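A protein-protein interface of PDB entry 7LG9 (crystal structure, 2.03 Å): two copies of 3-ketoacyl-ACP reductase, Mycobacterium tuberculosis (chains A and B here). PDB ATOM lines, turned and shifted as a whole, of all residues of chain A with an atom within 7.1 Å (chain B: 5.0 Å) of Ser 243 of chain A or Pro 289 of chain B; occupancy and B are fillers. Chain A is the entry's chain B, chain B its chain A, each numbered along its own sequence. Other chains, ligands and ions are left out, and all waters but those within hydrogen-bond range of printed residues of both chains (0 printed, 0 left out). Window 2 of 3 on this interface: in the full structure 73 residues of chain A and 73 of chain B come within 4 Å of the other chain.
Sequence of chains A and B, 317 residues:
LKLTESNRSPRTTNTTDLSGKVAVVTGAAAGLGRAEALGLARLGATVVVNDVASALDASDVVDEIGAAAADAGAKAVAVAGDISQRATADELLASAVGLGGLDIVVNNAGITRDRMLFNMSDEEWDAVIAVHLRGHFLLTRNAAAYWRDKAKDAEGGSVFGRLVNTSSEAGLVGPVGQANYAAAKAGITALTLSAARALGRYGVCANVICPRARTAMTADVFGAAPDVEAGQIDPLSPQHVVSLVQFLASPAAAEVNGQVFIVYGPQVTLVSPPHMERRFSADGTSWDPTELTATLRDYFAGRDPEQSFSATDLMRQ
No position is printed for both chains.
Of the 6 pairs that touch across the chains among the printed residues, none has its exchanged pair printed and touching as well.
Printed residues of chain A that touch a printed residue of chain B: Ser 243, Leu 244, Phe 247 and Val 268.
Hydrophobic or aromatic side chains of chain A within 4 Å of the printed part of chain B: Phe 247 and Val 268.
Of the 7 printed residues of chain B, 4 touch a printed residue of chain A.
Printed residues of chain B that touch a printed residue of chain A: Trp 287, Pro 289, Leu 292 and Thr 293.
Hydrophobic or aromatic side chains of chain B that line the printed part of chain A: Trp 287, Pro 289 and Leu 292.
Among the printed residues, no Asp or Glu carboxylate lies within 4 Å of a Lys or Arg side-chain nitrogen of the other chain.
The backbone carbonyl oxygen (O) of Pro 289 of chain B is in hydrogen-bond range of the side-chain hydroxyl (OG1) of Thr 293 of chain B (2.9 Å).
Among the printed residues, merely in contact across the chains: Ser 243 of chain A with Leu 292 of chain B (3.7 Å), Leu 244 of chain A with Leu 292 of chain B (3.7 Å), Phe 247 of chain A with Thr 293 of chain B (3.7 Å), Val 268 of chain A with Trp 287 of chain B (3.8 Å) and Ser 243 of chain A with Pro 289 of chain B (3.9 Å).
The backbone carbonyl oxygen (O) of Trp 287 of chain B is in hydrogen-bond range of the side-chain hydroxyl (OG) of Ser 243 of chain A (3.5 Å).
His 240 of chain A touches none of the printed residues of chain B.
Ser 243 of chain A touches just these residues of chain B: Trp 287 (3.5 Å), Pro 289 (3.9 Å) and Leu 292 (3.7 Å).
Printed residues of chain B within 4 Å of Val 268 of chain A: Trp 287.
Of the printed residues of chain A, Trp 287 of chain B touches Ser 243 and Val 268.
Printed residues of chain A within 4 Å of Leu 292 of chain B: Ser 243 (3.7 Å) and Leu 244 (3.7 Å).
Of the printed residues of chain A, Thr 293 of chain B touches Phe 247.
The nearest printed residue of chain A that does not touch Pro 289 of chain B is Gln 246 of chain A (4.003 Å).
The nearest printed residue of chain B that does not touch Val 268 of chain A is Leu 292 of chain B (4.1 Å).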
ATOM      1  N   THR A  16     -26.387  36.459   9.576  1.00  0.00           N
ATOM      2  CA  THR A  16     -25.462  36.503  10.703  1.00  0.00           C
ATOM      3  C   THR A  16     -24.942  37.920  10.927  1.00  0.00           C
ATOM      4  O   THR A  16     -23.850  38.115  11.463  1.00  0.00           O
ATOM      5  CB  THR A  16     -24.272  35.549  10.494  1.00  0.00           C
ATOM      6  N   LEU A  43     -24.248  41.146  17.321  1.00  0.00           N
ATOM      7  CA  LEU A  43     -24.417  41.135  15.874  1.00  0.00           C
ATOM      8  C   LEU A  43     -24.967  42.451  15.335  1.00  0.00           C
ATOM      9  O   LEU A  43     -25.299  42.529  14.148  1.00  0.00           O
ATOM     10  CB  LEU A  43     -25.325  39.975  15.460  1.00  0.00           C
ATOM     11  CG  LEU A  43     -24.784  38.585  15.804  1.00  0.00           C
ATOM     12  CD1 LEU A  43     -25.739  37.494  15.345  1.00  0.00           C
ATOM     13  CD2 LEU A  43     -23.404  38.383  15.197  1.00  0.00           C
ATOM     14  N   PRO A 238     -25.612  28.706  28.966  1.00  0.00           N
ATOM     15  CA  PRO A 238     -26.589  29.373  28.091  1.00  0.00           C
ATOM     16  C   PRO A 238     -26.046  29.717  26.716  1.00  0.00           C
ATOM     17  O   PRO A 238     -26.835  29.849  25.773  1.00  0.00           O
ATOM     18  CB  PRO A 238     -26.960  30.638  28.877  1.00  0.00           C
ATOM     19  CG  PRO A 238     -26.617  30.322  30.297  1.00  0.00           C
ATOM     20  CD  PRO A 238     -25.412  29.434  30.230  1.00  0.00           C
ATOM     21  N   GLN A 239     -24.727  29.860  26.568  1.00  0.00           N
ATOM     22  CA  GLN A 239     -24.143  30.240  25.287  1.00  0.00           C
ATOM     23  C   GLN A 239     -24.243  29.142  24.237  1.00  0.00           C
ATOM     24  O   GLN A 239     -24.023  29.424  23.053  1.00  0.00           O
ATOM     25  CB  GLN A 239     -22.682  30.648  25.486  1.00  0.00           C
ATOM     26  CG  GLN A 239     -22.515  31.956  26.242  1.00  0.00           C
ATOM     27  CD  GLN A 239     -21.062  32.349  26.421  1.00  0.00           C
ATOM     28  OE1 GLN A 239     -20.155  31.555  26.169  1.00  0.00           O
ATOM     29  NE2 GLN A 239     -20.832  33.583  26.858  1.00  0.00           N
ATOM     30  N   HIS A 240     -24.560  27.907  24.631  1.00  0.00           N
ATOM     31  CA  HIS A 240     -24.815  26.861  23.647  1.00  0.00           C
ATOM     32  C   HIS A 240     -26.107  27.103  22.879  1.00  0.00           C
ATOM     33  O   HIS A 240     -26.253  26.603  21.759  1.00  0.00           O
ATOM     34  CB  HIS A 240     -24.864  25.491  24.325  1.00  0.00           C
ATOM     35  CG  HIS A 240     -23.535  25.013  24.822  1.00  0.00           C
ATOM     36  ND1 HIS A 240     -22.563  24.513  23.982  1.00  0.00           N
ATOM     37  CD2 HIS A 240     -23.020  24.952  26.073  1.00  0.00           C
ATOM     38  CE1 HIS A 240     -21.504  24.168  24.693  1.00  0.00           C
ATOM     39  NE2 HIS A 240     -21.756  24.424  25.965  1.00  0.00           N
ATOM     40  N   VAL A 241     -27.043  27.854  23.455  1.00  0.00           N
ATOM     41  CA  VAL A 241     -28.287  28.183  22.772  1.00  0.00           C
ATOM     42  C   VAL A 241     -28.142  29.432  21.901  1.00  0.00           C
ATOM     43  O   VAL A 241     -28.825  29.556  20.878  1.00  0.00           O
ATOM     44  CB  VAL A 241     -29.413  28.344  23.813  1.00  0.00           C
ATOM     45  CG1 VAL A 241     -30.684  28.886  23.179  1.00  0.00           C
ATOM     46  CG2 VAL A 241     -29.695  27.014  24.496  1.00  0.00           C
ATOM     47  N   VAL A 242     -27.232  30.340  22.265  1.00  0.00           N
ATOM     48  CA  VAL A 242     -27.127  31.626  21.581  1.00  0.00           C
ATOM     49  C   VAL A 242     -26.785  31.437  20.109  1.00  0.00           C
ATOM     50  O   VAL A 242     -27.306  32.151  19.242  1.00  0.00           O
ATOM     51  CB  VAL A 242     -26.096  32.521  22.293  1.00  0.00           C
ATOM     52  CG1 VAL A 242     -25.966  33.861  21.585  1.00  0.00           C
ATOM     53  CG2 VAL A 242     -26.487  32.718  23.747  1.00  0.00           C
ATOM     54  N   SER A 243     -25.911  30.475  19.799  1.00  0.00           N
ATOM     55  CA  SER A 243     -25.520  30.250  18.410  1.00  0.00           C
ATOM     56  C   SER A 243     -26.727  29.934  17.534  1.00  0.00           C
ATOM     57  O   SER A 243     -26.820  30.412  16.396  1.00  0.00           O
ATOM     58  CB  SER A 243     -24.491  29.123  18.326  1.00  0.00           C
ATOM     59  OG  SER A 243     -23.231  29.541  18.820  1.00  0.00           O
ATOM     60  N   LEU A 244     -27.667  29.136  18.045  1.00  0.00           N
ATOM     61  CA  LEU A 244     -28.862  28.826  17.268  1.00  0.00           C
ATOM     62  C   LEU A 244     -29.816  30.013  17.221  1.00  0.00           C
ATOM     63  O   LEU A 244     -30.394  30.308  16.168  1.00  0.00           O
ATOM     64  CB  LEU A 244     -29.562  27.598  17.843  1.00  0.00           C
ATOM     65  CG  LEU A 244     -30.826  27.188  17.089  1.00  0.00           C
ATOM     66  CD1 LEU A 244     -30.521  26.986  15.615  1.00  0.00           C
ATOM     67  CD2 LEU A 244     -31.418  25.935  17.687  1.00  0.00           C
ATOM     68  N   VAL A 245     -30.000  30.699  18.352  1.00  0.00           N
ATOM     69  CA  VAL A 245     -30.879  31.865  18.383  1.00  0.00           C
ATOM     70  C   VAL A 245     -30.376  32.937  17.423  1.00  0.00           C
ATOM     71  O   VAL A 245     -31.167  33.625  16.767  1.00  0.00           O
ATOM     72  CB  VAL A 245     -31.003  32.399  19.824  1.00  0.00           C
ATOM     73  CG1 VAL A 245     -31.799  33.694  19.855  1.00  0.00           C
ATOM     74  CG2 VAL A 245     -31.655  31.355  20.715  1.00  0.00           C
ATOM     75  N   GLN A 246     -29.054  33.087  17.316  1.00  0.00           N
ATOM     76  CA  GLN A 246     -28.497  34.037  16.358  1.00  0.00           C
ATOM     77  C   GLN A 246     -28.823  33.629  14.927  1.00  0.00           C
ATOM     78  O   GLN A 246     -29.099  34.484  14.077  1.00  0.00           O
ATOM     79  CB  GLN A 246     -26.988  34.156  16.557  1.00  0.00           C
ATOM     80  CG  GLN A 246     -26.585  34.919  17.809  1.00  0.00           C
ATOM     81  CD  GLN A 246     -25.088  34.898  18.046  1.00  0.00           C
ATOM     82  OE1 GLN A 246     -24.417  33.907  17.757  1.00  0.00           O
ATOM     83  NE2 GLN A 246     -24.556  35.995  18.569  1.00  0.00           N
ATOM     84  N   PHE A 247     -28.797  32.325  14.641  1.00  0.00           N
ATOM     85  CA  PHE A 247     -29.185  31.854  13.316  1.00  0.00           C
ATOM     86  C   PHE A 247     -30.675  32.055  13.076  1.00  0.00           C
ATOM     87  O   PHE A 247     -31.078  32.614  12.050  1.00  0.00           O
ATOM     88  CB  PHE A 247     -28.815  30.381  13.145  1.00  0.00           C
ATOM     89  CG  PHE A 247     -29.387  29.757  11.902  1.00  0.00           C
ATOM     90  CD1 PHE A 247     -28.948  30.152  10.650  1.00  0.00           C
ATOM     91  CD2 PHE A 247     -30.365  28.777  11.986  1.00  0.00           C
ATOM     92  CE1 PHE A 247     -29.473  29.581   9.503  1.00  0.00           C
ATOM     93  CE2 PHE A 247     -30.892  28.201  10.844  1.00  0.00           C
ATOM     94  CZ  PHE A 247     -30.446  28.603   9.601  1.00  0.00           C
ATOM     95  N   LEU A 248     -31.511  31.606  14.018  1.00  0.00           N
ATOM     96  CA  LEU A 248     -32.957  31.681  13.832  1.00  0.00           C
ATOM     97  C   LEU A 248     -33.465  33.114  13.786  1.00  0.00           C
ATOM     98  O   LEU A 248     -34.609  33.342  13.375  1.00  0.00           O
ATOM     99  CB  LEU A 248     -33.673  30.918  14.947  1.00  0.00           C
ATOM    100  CG  LEU A 248     -33.437  29.408  15.012  1.00  0.00           C
ATOM    101  CD1 LEU A 248     -34.280  28.784  16.113  1.00  0.00           C
ATOM    102  CD2 LEU A 248     -33.736  28.759  13.671  1.00  0.00           C
ATOM    103  N   VAL A 268     -27.159  20.103  18.159  1.00  0.00           N
ATOM    104  CA  VAL A 268     -28.409  20.747  17.769  1.00  0.00           C
ATOM    105  C   VAL A 268     -29.242  19.698  17.049  1.00  0.00           C
ATOM    106  O   VAL A 268     -28.877  19.252  15.953  1.00  0.00           O
ATOM    107  CB  VAL A 268     -28.181  21.977  16.882  1.00  0.00           C
ATOM    108  CG1 VAL A 268     -29.516  22.560  16.439  1.00  0.00           C
ATOM    109  CG2 VAL A 268     -27.358  23.018  17.620  1.00  0.00           C
ATOM    110  N   TRP B 287     -20.522  24.858  19.163  1.00  0.00           N
ATOM    111  CA  TRP B 287     -20.785  25.236  17.781  1.00  0.00           C
ATOM    112  C   TRP B 287     -20.225  26.623  17.500  1.00  0.00           C
ATOM    113  O   TRP B 287     -20.436  27.558  18.278  1.00  0.00           O
ATOM    114  CB  TRP B 287     -22.288  25.221  17.497  1.00  0.00           C
ATOM    115  CG  TRP B 287     -22.793  23.950  16.894  1.00  0.00           C
ATOM    116  CD1 TRP B 287     -23.578  23.014  17.498  1.00  0.00           C
ATOM    117  CD2 TRP B 287     -22.556  23.478  15.561  1.00  0.00           C
ATOM    118  NE1 TRP B 287     -23.844  21.984  16.626  1.00  0.00           N
ATOM    119  CE2 TRP B 287     -23.226  22.246  15.430  1.00  0.00           C
ATOM    120  CE3 TRP B 287     -21.839  23.976  14.469  1.00  0.00           C
ATOM    121  CZ2 TRP B 287     -23.202  21.504  14.249  1.00  0.00           C
ATOM    122  CZ3 TRP B 287     -21.818  23.238  13.298  1.00  0.00           C
ATOM    123  CH2 TRP B 287     -22.494  22.017  13.197  1.00  0.00           C
ATOM    124  N   ASP B 288     -19.505  26.753  16.395  1.00  0.00           N
ATOM    125  CA  ASP B 288     -19.185  28.093  15.926  1.00  0.00           C
ATOM    126  C   ASP B 288     -20.412  28.698  15.244  1.00  0.00           C
ATOM    127  O   ASP B 288     -21.113  28.001  14.504  1.00  0.00           O
ATOM    128  CB  ASP B 288     -18.005  28.061  14.957  1.00  0.00           C
ATOM    129  CG  ASP B 288     -17.857  29.353  14.179  1.00  0.00           C
ATOM    130  OD1 ASP B 288     -17.316  30.332  14.734  1.00  0.00           O
ATOM    131  OD2 ASP B 288     -18.291  29.388  13.009  1.00  0.00           O
ATOM    132  N   PRO B 289     -20.706  29.976  15.496  1.00  0.00           N
ATOM    133  CA  PRO B 289     -21.914  30.581  14.904  1.00  0.00           C
ATOM    134  C   PRO B 289     -21.997  30.450  13.391  1.00  0.00           C
ATOM    135  O   PRO B 289     -23.023  29.991  12.870  1.00  0.00           O
ATOM    136  CB  PRO B 289     -21.812  32.044  15.355  1.00  0.00           C
ATOM    137  CG  PRO B 289     -21.050  31.980  16.634  1.00  0.00           C
ATOM    138  CD  PRO B 289     -20.045  30.878  16.456  1.00  0.00           C
ATOM    139  N   THR B 290     -20.942  30.832  12.666  1.00  0.00           N
ATOM    140  CA  THR B 290     -20.967  30.703  11.212  1.00  0.00           C
ATOM    141  C   THR B 290     -20.934  29.243  10.778  1.00  0.00           C
ATOM    142  O   THR B 290     -21.536  28.885   9.760  1.00  0.00           O
ATOM    143  CB  THR B 290     -19.792  31.461  10.589  1.00  0.00           C
ATOM    144  OG1 THR B 290     -18.581  30.729  10.809  1.00  0.00           O
ATOM    145  CG2 THR B 290     -19.654  32.843  11.211  1.00  0.00           C
ATOM    146  N   GLU B 291     -20.234  28.390  11.530  1.00  0.00           N
ATOM    147  CA  GLU B 291     -20.221  26.965  11.219  1.00  0.00           C
ATOM    148  C   GLU B 291     -21.616  26.365  11.339  1.00  0.00           C
ATOM    149  O   GLU B 291     -22.022  25.542  10.509  1.00  0.00           O
ATOM    150  CB  GLU B 291     -19.243  26.246  12.145  1.00  0.00           C
ATOM    151  CG  GLU B 291     -19.048  24.773  11.840  1.00  0.00           C
ATOM    152  CD  GLU B 291     -18.219  24.066  12.898  1.00  0.00           C
ATOM    153  OE1 GLU B 291     -17.815  24.728  13.876  1.00  0.00           O
ATOM    154  OE2 GLU B 291     -17.972  22.850  12.755  1.00  0.00           O
ATOM    155  N   LEU B 292     -22.358  26.760  12.373  1.00  0.00           N
ATOM    156  CA  LEU B 292     -23.729  26.285  12.525  1.00  0.00           C
ATOM    157  C   LEU B 292     -24.636  26.867  11.448  1.00  0.00           C
ATOM    158  O   LEU B 292     -25.492  26.160  10.903  1.00  0.00           O
ATOM    159  CB  LEU B 292     -24.254  26.638  13.915  1.00  0.00           C
ATOM    160  CG  LEU B 292     -25.721  26.293  14.170  1.00  0.00           C
ATOM    161  CD1 LEU B 292     -25.916  24.786  14.199  1.00  0.00           C
ATOM    162  CD2 LEU B 292     -26.210  26.931  15.461  1.00  0.00           C
ATOM    163  N   THR B 293     -24.466  28.154  11.131  1.00  0.00           N
ATOM    164  CA  THR B 293     -25.288  28.779  10.099  1.00  0.00           C
ATOM    165  C   THR B 293     -25.119  28.078   8.758  1.00  0.00           C
ATOM    166  O   THR B 293     -26.101  27.844   8.045  1.00  0.00           O
ATOM    167  CB  THR B 293     -24.941  30.264   9.977  1.00  0.00           C
ATOM    168  OG1 THR B 293     -25.222  30.924  11.218  1.00  0.00           O
ATOM    169  CG2 THR B 293     -25.759  30.922   8.872  1.00  0.00           C
